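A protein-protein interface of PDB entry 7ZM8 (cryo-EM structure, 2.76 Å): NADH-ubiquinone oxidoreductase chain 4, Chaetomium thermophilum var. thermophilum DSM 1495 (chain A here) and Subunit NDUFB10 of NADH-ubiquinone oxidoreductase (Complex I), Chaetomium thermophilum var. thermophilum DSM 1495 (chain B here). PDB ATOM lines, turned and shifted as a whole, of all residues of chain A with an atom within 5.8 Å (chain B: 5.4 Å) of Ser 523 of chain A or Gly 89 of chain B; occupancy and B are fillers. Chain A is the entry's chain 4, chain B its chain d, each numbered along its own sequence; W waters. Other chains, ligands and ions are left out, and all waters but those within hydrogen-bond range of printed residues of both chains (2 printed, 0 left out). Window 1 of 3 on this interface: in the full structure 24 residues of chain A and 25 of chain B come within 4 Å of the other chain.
O of Val 87 of chain B touches CG1 of Ile 363 of chain A, at 3.8 Å.
His 519 of chain A touches Trp 43 of chain B (ND1 to CH2, 3.8 Å).
Tyr 520 of chain A touches Ile 39 of chain B.
Ser 523 of chain A touches Ile 39 of chain B (O to CD1, 3.6 Å).
Ser 523 of chain A touches Val 87 of chain B.
O of Ser 523 of chain A touches CA of Gly 89 of chain B, at 3.3 Å.
Ser 524 of chain A touches Tyr 90 of chain B (CB to OH, 3.4 Å).
Val 526 of chain A touches Leu 91 of chain B.
Of the 10 printed residues of chain B, 7 touch a printed residue of chain A.
Hydrophobic or aromatic side chains of chain B that line the printed part of chain A: Ile 39, Trp 43, Val 87, Tyr 90 and Leu 91.
Of the 11 printed residues of chain A, 7 touch a printed residue of chain B.
Among the printed residues, 11 pairs touch across the chains.
O of Gly 528 of chain A lies close to O of Lys 88 of chain B (3.4 Å).
The backbone carbonyl oxygen (O) of Lys 88 of chain B sits close to the backbone carbonyl oxygen (O) of Val 526 of chain A (3.1 Å).
The indole nitrogen (NE1) of Trp 43 of chain B sits at hydrogen-bond distance from the side-chain hydroxyl (OG) of Ser 523 of chain A, at 2.8 Å.
Water W2 lies within hydrogen-bond range of the backbone carbonyl oxygen (O) of Lys 88 of chain B (2.6 Å), the backbone carbonyl oxygen (O) of Val 526 of chain A (2.7 Å), the backbone NH (N) of Gly 528 of chain A (2.8 Å) and the backbone NH (N) of Leu 91 of chain B (3.4 Å).
Water W1 lies within hydrogen-bond range of the backbone carbonyl oxygen (O) of Ser 524 of chain A, the backbone NH (N) of Tyr 90 of chain B, the backbone carbonyl oxygen (O) of Val 526 of chain A and the backbone NH (N) of Leu 91 of chain B.
Ser 523 of chain A touches just these residues of chain B: Ile 39 (3.6 Å), Trp 43 (2.8 Å), Val 87 (3.5 Å) and Gly 89 (3.3 Å).
Gly 89 of chain B touches one residue of chain A.
Printed residues of chain A within 4 Å of Trp 43 of chain B: His 519 (3.8 Å) and Ser 523 (2.8 Å).
Printed residues of chain B within 4 Å of Ser 524 of chain A: Tyr 90.
Of the printed residues of chain A, Lys 88 of chain B touches Val 526 and Gly 528.
Printed residues of chain B within 4 Å of Ile 363 of chain A: Val 87 (3.8 Å).
Of the printed residues of chain B, His 519 of chain A touches Trp 43 (3.8 Å).
Gln 42 of chain B touches none of the printed residues of chain A.
Glu 93 of chain B touches none of the printed residues of chain A.
The nearest residue of chain B that does not touch Ser 523 of chain A is Tyr 90 of chain B (4.7 Å).
The nearest residue of chain A that does not touch Gly 89 of chain B is Val 526 of chain A (4.04 Å).
The backbone NH (N) of Lys 88 of chain B is in hydrogen-bond range of the side-chain amide oxygen (OE1) of Gln 42 of chain B (3.2 Å).
The side-chain amide nitrogen (NE2) of Gln 42 of chain B sits at hydrogen-bond distance from the backbone carbonyl oxygen (O) of Gly 89 of chain B.
The backbone carbonyl oxygen (O) of His 519 of chain A sits at hydrogen-bond distance from the side-chain hydroxyl (OG) of Ser 523 of chain A (2.8 Å).
The side-chain hydroxyl (OG) of Ser 524 of chain A is in hydrogen-bond range of the backbone carbonyl oxygen (O) of Asn 521 of chain A, 2.6 Å away.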
ATOM      1  N   ILE A 363     -11.041 -25.415 -25.267  1.00  0.00           N
ATOM      2  CA  ILE A 363     -11.677 -25.004 -26.544  1.00  0.00           C
ATOM      3  C   ILE A 363     -10.558 -24.615 -27.496  1.00  0.00           C
ATOM      4  O   ILE A 363     -10.694 -24.923 -28.685  1.00  0.00           O
ATOM      5  CB  ILE A 363     -12.641 -23.830 -26.308  1.00  0.00           C
ATOM      6  CG1 ILE A 363     -13.999 -24.297 -25.785  1.00  0.00           C
ATOM      7  CG2 ILE A 363     -12.787 -22.994 -27.568  1.00  0.00           C
ATOM      8  CD1 ILE A 363     -14.930 -24.786 -26.866  1.00  0.00           C
ATOM      9  N   LEU A 518     -16.289 -23.943 -36.512  1.00  0.00           N
ATOM     10  CA  LEU A 518     -16.029 -24.949 -35.447  1.00  0.00           C
ATOM     11  C   LEU A 518     -16.464 -24.533 -34.040  1.00  0.00           C
ATOM     12  O   LEU A 518     -16.705 -25.433 -33.253  1.00  0.00           O
ATOM     13  CB  LEU A 518     -14.516 -25.186 -35.386  1.00  0.00           C
ATOM     14  CG  LEU A 518     -13.809 -25.652 -36.651  1.00  0.00           C
ATOM     15  CD1 LEU A 518     -12.314 -25.447 -36.497  1.00  0.00           C
ATOM     16  CD2 LEU A 518     -14.108 -27.112 -36.923  1.00  0.00           C
ATOM     17  N   HIS A 519     -16.560 -23.243 -33.730  1.00  0.00           N
ATOM     18  CA  HIS A 519     -16.821 -22.770 -32.337  1.00  0.00           C
ATOM     19  C   HIS A 519     -17.940 -23.519 -31.606  1.00  0.00           C
ATOM     20  O   HIS A 519     -17.629 -24.124 -30.572  1.00  0.00           O
ATOM     21  CB  HIS A 519     -17.083 -21.260 -32.336  1.00  0.00           C
ATOM     22  CG  HIS A 519     -15.862 -20.421 -32.488  1.00  0.00           C
ATOM     23  ND1 HIS A 519     -14.733 -20.625 -31.728  1.00  0.00           N
ATOM     24  CD2 HIS A 519     -15.596 -19.367 -33.285  1.00  0.00           C
ATOM     25  CE1 HIS A 519     -13.816 -19.746 -32.069  1.00  0.00           C
ATOM     26  NE2 HIS A 519     -14.322 -18.960 -33.018  1.00  0.00           N
ATOM     27  N   TYR A 520     -19.179 -23.459 -32.096  1.00  0.00           N
ATOM     28  CA  TYR A 520     -20.366 -24.047 -31.432  1.00  0.00           C
ATOM     29  C   TYR A 520     -20.246 -25.571 -31.343  1.00  0.00           C
ATOM     30  O   TYR A 520     -20.615 -26.149 -30.319  1.00  0.00           O
ATOM     31  CB  TYR A 520     -21.592 -23.580 -32.212  1.00  0.00           C
ATOM     32  CG  TYR A 520     -22.911 -24.049 -31.670  1.00  0.00           C
ATOM     33  CD1 TYR A 520     -23.562 -23.341 -30.678  1.00  0.00           C
ATOM     34  CD2 TYR A 520     -23.503 -25.198 -32.155  1.00  0.00           C
ATOM     35  CE1 TYR A 520     -24.771 -23.767 -30.165  1.00  0.00           C
ATOM     36  CE2 TYR A 520     -24.710 -25.639 -31.652  1.00  0.00           C
ATOM     37  CZ  TYR A 520     -25.342 -24.923 -30.657  1.00  0.00           C
ATOM     38  OH  TYR A 520     -26.532 -25.365 -30.172  1.00  0.00           O
ATOM     39  N   ASN A 521     -19.813 -26.209 -32.418  1.00  0.00           N
ATOM     40  CA  ASN A 521     -19.668 -27.687 -32.476  1.00  0.00           C
ATOM     41  C   ASN A 521     -18.504 -28.168 -31.601  1.00  0.00           C
ATOM     42  O   ASN A 521     -18.593 -29.278 -31.084  1.00  0.00           O
ATOM     43  CB  ASN A 521     -19.725 -28.194 -33.921  1.00  0.00           C
ATOM     44  CG  ASN A 521     -21.035 -27.861 -34.610  1.00  0.00           C
ATOM     45  OD1 ASN A 521     -21.047 -27.450 -35.762  1.00  0.00           O
ATOM     46  ND2 ASN A 521     -22.148 -28.012 -33.916  1.00  0.00           N
ATOM     47  N   ILE A 522     -17.413 -27.414 -31.522  1.00  0.00           N
ATOM     48  CA  ILE A 522     -16.287 -27.760 -30.616  1.00  0.00           C
ATOM     49  C   ILE A 522     -16.816 -27.640 -29.191  1.00  0.00           C
ATOM     50  O   ILE A 522     -16.397 -28.422 -28.331  1.00  0.00           O
ATOM     51  CB  ILE A 522     -15.041 -26.880 -30.892  1.00  0.00           C
ATOM     52  CG1 ILE A 522     -14.386 -27.216 -32.234  1.00  0.00           C
ATOM     53  CG2 ILE A 522     -14.030 -26.964 -29.760  1.00  0.00           C
ATOM     54  CD1 ILE A 522     -13.479 -28.409 -32.187  1.00  0.00           C
ATOM     55  N   SER A 523     -17.734 -26.714 -28.962  1.00  0.00           N
ATOM     56  CA  SER A 523     -18.222 -26.459 -27.589  1.00  0.00           C
ATOM     57  C   SER A 523     -18.858 -27.721 -27.032  1.00  0.00           C
ATOM     58  O   SER A 523     -18.921 -27.835 -25.810  1.00  0.00           O
ATOM     59  CB  SER A 523     -19.162 -25.290 -27.566  1.00  0.00           C
ATOM     60  OG  SER A 523     -18.477 -24.115 -27.950  1.00  0.00           O
ATOM     61  N   SER A 524     -19.324 -28.612 -27.891  1.00  0.00           N
ATOM     62  CA  SER A 524     -20.031 -29.840 -27.462  1.00  0.00           C
ATOM     63  C   SER A 524     -19.097 -30.962 -26.988  1.00  0.00           C
ATOM     64  O   SER A 524     -19.620 -31.925 -26.436  1.00  0.00           O
ATOM     65  CB  SER A 524     -20.945 -30.301 -28.552  1.00  0.00           C
ATOM     66  OG  SER A 524     -20.218 -30.784 -29.669  1.00  0.00           O
ATOM     67  N   VAL A 525     -17.785 -30.885 -27.215  1.00  0.00           N
ATOM     68  CA  VAL A 525     -16.874 -32.018 -26.848  1.00  0.00           C
ATOM     69  C   VAL A 525     -16.047 -31.709 -25.595  1.00  0.00           C
ATOM     70  O   VAL A 525     -15.189 -32.526 -25.274  1.00  0.00           O
ATOM     71  CB  VAL A 525     -15.977 -32.496 -28.013  1.00  0.00           C
ATOM     72  CG1 VAL A 525     -16.733 -33.342 -29.022  1.00  0.00           C
ATOM     73  CG2 VAL A 525     -15.236 -31.359 -28.692  1.00  0.00           C
ATOM     74  N   VAL A 526     -16.293 -30.585 -24.922  1.00  0.00           N
ATOM     75  CA  VAL A 526     -15.523 -30.201 -23.696  1.00  0.00           C
ATOM     76  C   VAL A 526     -16.132 -30.914 -22.494  1.00  0.00           C
ATOM     77  O   VAL A 526     -17.358 -30.979 -22.438  1.00  0.00           O
ATOM     78  CB  VAL A 526     -15.316 -28.686 -23.518  1.00  0.00           C
ATOM     79  CG1 VAL A 526     -14.413 -28.378 -22.336  1.00  0.00           C
ATOM     80  CG2 VAL A 526     -14.775 -28.041 -24.780  1.00  0.00           C
ATOM     81  N   GLY A 528     -16.359 -30.716 -18.408  1.00  0.00           N
ATOM     82  CA  GLY A 528     -16.045 -29.981 -17.190  1.00  0.00           C
ATOM     83  C   GLY A 528     -17.127 -29.034 -16.781  1.00  0.00           C
ATOM     84  O   GLY A 528     -17.997 -28.760 -17.581  1.00  0.00           O
ATOM     85  N   ILE B  38     -27.623 -24.507 -22.767  1.00  0.00           N
ATOM     86  CA  ILE B  38     -26.431 -24.396 -21.885  1.00  0.00           C
ATOM     87  C   ILE B  38     -25.250 -23.795 -22.649  1.00  0.00           C
ATOM     88  O   ILE B  38     -24.591 -22.906 -22.101  1.00  0.00           O
ATOM     89  CB  ILE B  38     -26.151 -25.762 -21.234  1.00  0.00           C
ATOM     90  CG1 ILE B  38     -27.305 -26.173 -20.321  1.00  0.00           C
ATOM     91  CG2 ILE B  38     -24.821 -25.779 -20.500  1.00  0.00           C
ATOM     92  CD1 ILE B  38     -27.008 -27.353 -19.449  1.00  0.00           C
ATOM     93  N   ILE B  39     -25.031 -24.221 -23.885  1.00  0.00           N
ATOM     94  CA  ILE B  39     -23.872 -23.729 -24.684  1.00  0.00           C
ATOM     95  C   ILE B  39     -24.054 -22.235 -24.944  1.00  0.00           C
ATOM     96  O   ILE B  39     -23.055 -21.517 -24.875  1.00  0.00           O
ATOM     97  CB  ILE B  39     -23.717 -24.546 -25.989  1.00  0.00           C
ATOM     98  CG1 ILE B  39     -23.380 -26.012 -25.714  1.00  0.00           C
ATOM     99  CG2 ILE B  39     -22.707 -23.908 -26.927  1.00  0.00           C
ATOM    100  CD1 ILE B  39     -22.058 -26.221 -25.027  1.00  0.00           C
ATOM    101  N   GLN B  42     -23.189 -20.079 -21.783  1.00  0.00           N
ATOM    102  CA  GLN B  42     -21.733 -20.050 -21.506  1.00  0.00           C
ATOM    103  C   GLN B  42     -21.089 -19.065 -22.476  1.00  0.00           C
ATOM    104  O   GLN B  42     -20.209 -18.318 -22.050  1.00  0.00           O
ATOM    105  CB  GLN B  42     -21.118 -21.436 -21.651  1.00  0.00           C
ATOM    106  CG  GLN B  42     -21.581 -22.436 -20.607  1.00  0.00           C
ATOM    107  CD  GLN B  42     -21.066 -23.815 -20.922  1.00  0.00           C
ATOM    108  OE1 GLN B  42     -20.396 -24.032 -21.925  1.00  0.00           O
ATOM    109  NE2 GLN B  42     -21.369 -24.763 -20.055  1.00  0.00           N
ATOM    110  N   TRP B  43     -21.530 -19.065 -23.725  1.00  0.00           N
ATOM    111  CA  TRP B  43     -21.012 -18.151 -24.763  1.00  0.00           C
ATOM    112  C   TRP B  43     -21.395 -16.686 -24.526  1.00  0.00           C
ATOM    113  O   TRP B  43     -20.579 -15.819 -24.847  1.00  0.00           O
ATOM    114  CB  TRP B  43     -21.450 -18.672 -26.125  1.00  0.00           C
ATOM    115  CG  TRP B  43     -20.499 -19.655 -26.728  1.00  0.00           C
ATOM    116  CD1 TRP B  43     -20.635 -21.008 -26.776  1.00  0.00           C
ATOM    117  CD2 TRP B  43     -19.251 -19.356 -27.373  1.00  0.00           C
ATOM    118  NE1 TRP B  43     -19.565 -21.570 -27.410  1.00  0.00           N
ATOM    119  CE2 TRP B  43     -18.697 -20.584 -27.784  1.00  0.00           C
ATOM    120  CE3 TRP B  43     -18.553 -18.178 -27.646  1.00  0.00           C
ATOM    121  CZ2 TRP B  43     -17.477 -20.667 -28.448  1.00  0.00           C
ATOM    122  CZ3 TRP B  43     -17.347 -18.262 -28.304  1.00  0.00           C
ATOM    123  CH2 TRP B  43     -16.818 -19.489 -28.698  1.00  0.00           C
ATOM    124  N   VAL B  87     -16.027 -21.765 -21.592  1.00  0.00           N
ATOM    125  CA  VAL B  87     -17.012 -22.613 -22.308  1.00  0.00           C
ATOM    126  C   VAL B  87     -16.626 -24.038 -21.929  1.00  0.00           C
ATOM    127  O   VAL B  87     -15.567 -24.499 -22.365  1.00  0.00           O
ATOM    128  CB  VAL B  87     -17.093 -22.309 -23.818  1.00  0.00           C
ATOM    129  CG1 VAL B  87     -17.869 -23.382 -24.558  1.00  0.00           C
ATOM    130  CG2 VAL B  87     -17.680 -20.934 -24.092  1.00  0.00           C
ATOM    131  N   LYS B  88     -17.417 -24.666 -21.064  1.00  0.00           N
ATOM    132  CA  LYS B  88     -17.032 -25.991 -20.522  1.00  0.00           C
ATOM    133  C   LYS B  88     -17.867 -27.092 -21.153  1.00  0.00           C
ATOM    134  O   LYS B  88     -17.531 -28.242 -20.943  1.00  0.00           O
ATOM    135  CB  LYS B  88     -17.116 -25.941 -18.996  1.00  0.00           C
ATOM    136  CG  LYS B  88     -16.152 -24.978 -18.320  1.00  0.00           C
ATOM    137  CD  LYS B  88     -14.708 -25.388 -18.467  1.00  0.00           C
ATOM    138  CE  LYS B  88     -14.425 -26.735 -17.841  1.00  0.00           C
ATOM    139  NZ  LYS B  88     -13.087 -27.249 -18.213  1.00  0.00           N
ATOM    140  N   GLY B  89     -18.871 -26.731 -21.927  1.00  0.00           N
ATOM    141  CA  GLY B  89     -19.738 -27.718 -22.582  1.00  0.00           C
ATOM    142  C   GLY B  89     -20.906 -28.170 -21.731  1.00  0.00           C
ATOM    143  O   GLY B  89     -21.084 -27.601 -20.651  1.00  0.00           O
ATOM    144  N   TYR B  90     -21.687 -29.139 -22.215  1.00  0.00           N
ATOM    145  CA  TYR B  90     -22.798 -29.715 -21.476  1.00  0.00           C
ATOM    146  C   TYR B  90     -22.531 -31.139 -21.020  1.00  0.00           C
ATOM    147  O   TYR B  90     -23.318 -31.679 -20.241  1.00  0.00           O
ATOM    148  CB  TYR B  90     -24.068 -29.692 -22.340  1.00  0.00           C
ATOM    149  CG  TYR B  90     -23.914 -30.374 -23.683  1.00  0.00           C
ATOM    150  CD1 TYR B  90     -23.908 -31.760 -23.790  1.00  0.00           C
ATOM    151  CD2 TYR B  90     -23.781 -29.634 -24.842  1.00  0.00           C
ATOM    152  CE1 TYR B  90     -23.763 -32.377 -25.000  1.00  0.00           C
ATOM    153  CE2 TYR B  90     -23.640 -30.248 -26.060  1.00  0.00           C
ATOM    154  CZ  TYR B  90     -23.635 -31.620 -26.133  1.00  0.00           C
ATOM    155  OH  TYR B  90     -23.494 -32.242 -27.348  1.00  0.00           O
ATOM    156  N   LEU B  91     -21.441 -31.746 -21.477  1.00  0.00           N
ATOM    157  CA  LEU B  91     -21.261 -33.187 -21.351  1.00  0.00           C
ATOM    158  C   LEU B  91     -21.203 -33.616 -19.894  1.00  0.00           C
ATOM    159  O   LEU B  91     -21.840 -34.596 -19.502  1.00  0.00           O
ATOM    160  CB  LEU B  91     -19.991 -33.595 -22.087  1.00  0.00           C
ATOM    161  CG  LEU B  91     -19.836 -35.028 -22.564  1.00  0.00           C
ATOM    162  CD1 LEU B  91     -20.974 -35.397 -23.492  1.00  0.00           C
ATOM    163  CD2 LEU B  91     -18.499 -35.140 -23.260  1.00  0.00           C
ATOM    164  N   GLU B  93     -22.408 -31.751 -17.452  1.00  0.00           N
ATOM    165  CA  GLU B  93     -23.705 -31.338 -16.934  1.00  0.00           C
ATOM    166  C   GLU B  93     -24.777 -32.361 -17.280  1.00  0.00           C
ATOM    167  O   GLU B  93     -25.638 -32.679 -16.455  1.00  0.00           O
ATOM    168  CB  GLU B  93     -24.045 -29.971 -17.522  1.00  0.00           C
ATOM    169  CG  GLU B  93     -25.326 -29.326 -17.078  1.00  0.00           C
ATOM    170  CD  GLU B  93     -25.320 -28.966 -15.618  1.00  0.00           C
ATOM    171  OE1 GLU B  93     -24.224 -28.759 -15.068  1.00  0.00           O
ATOM    172  OE2 GLU B  93     -26.416 -28.839 -15.040  1.00  0.00           O
HETATM  173  O   HOH W   1     -19.989 -30.804 -24.076  1.00  0.00           O
HETATM  174  O   HOH W   2     -18.593 -30.480 -20.051  1.00  0.00           O
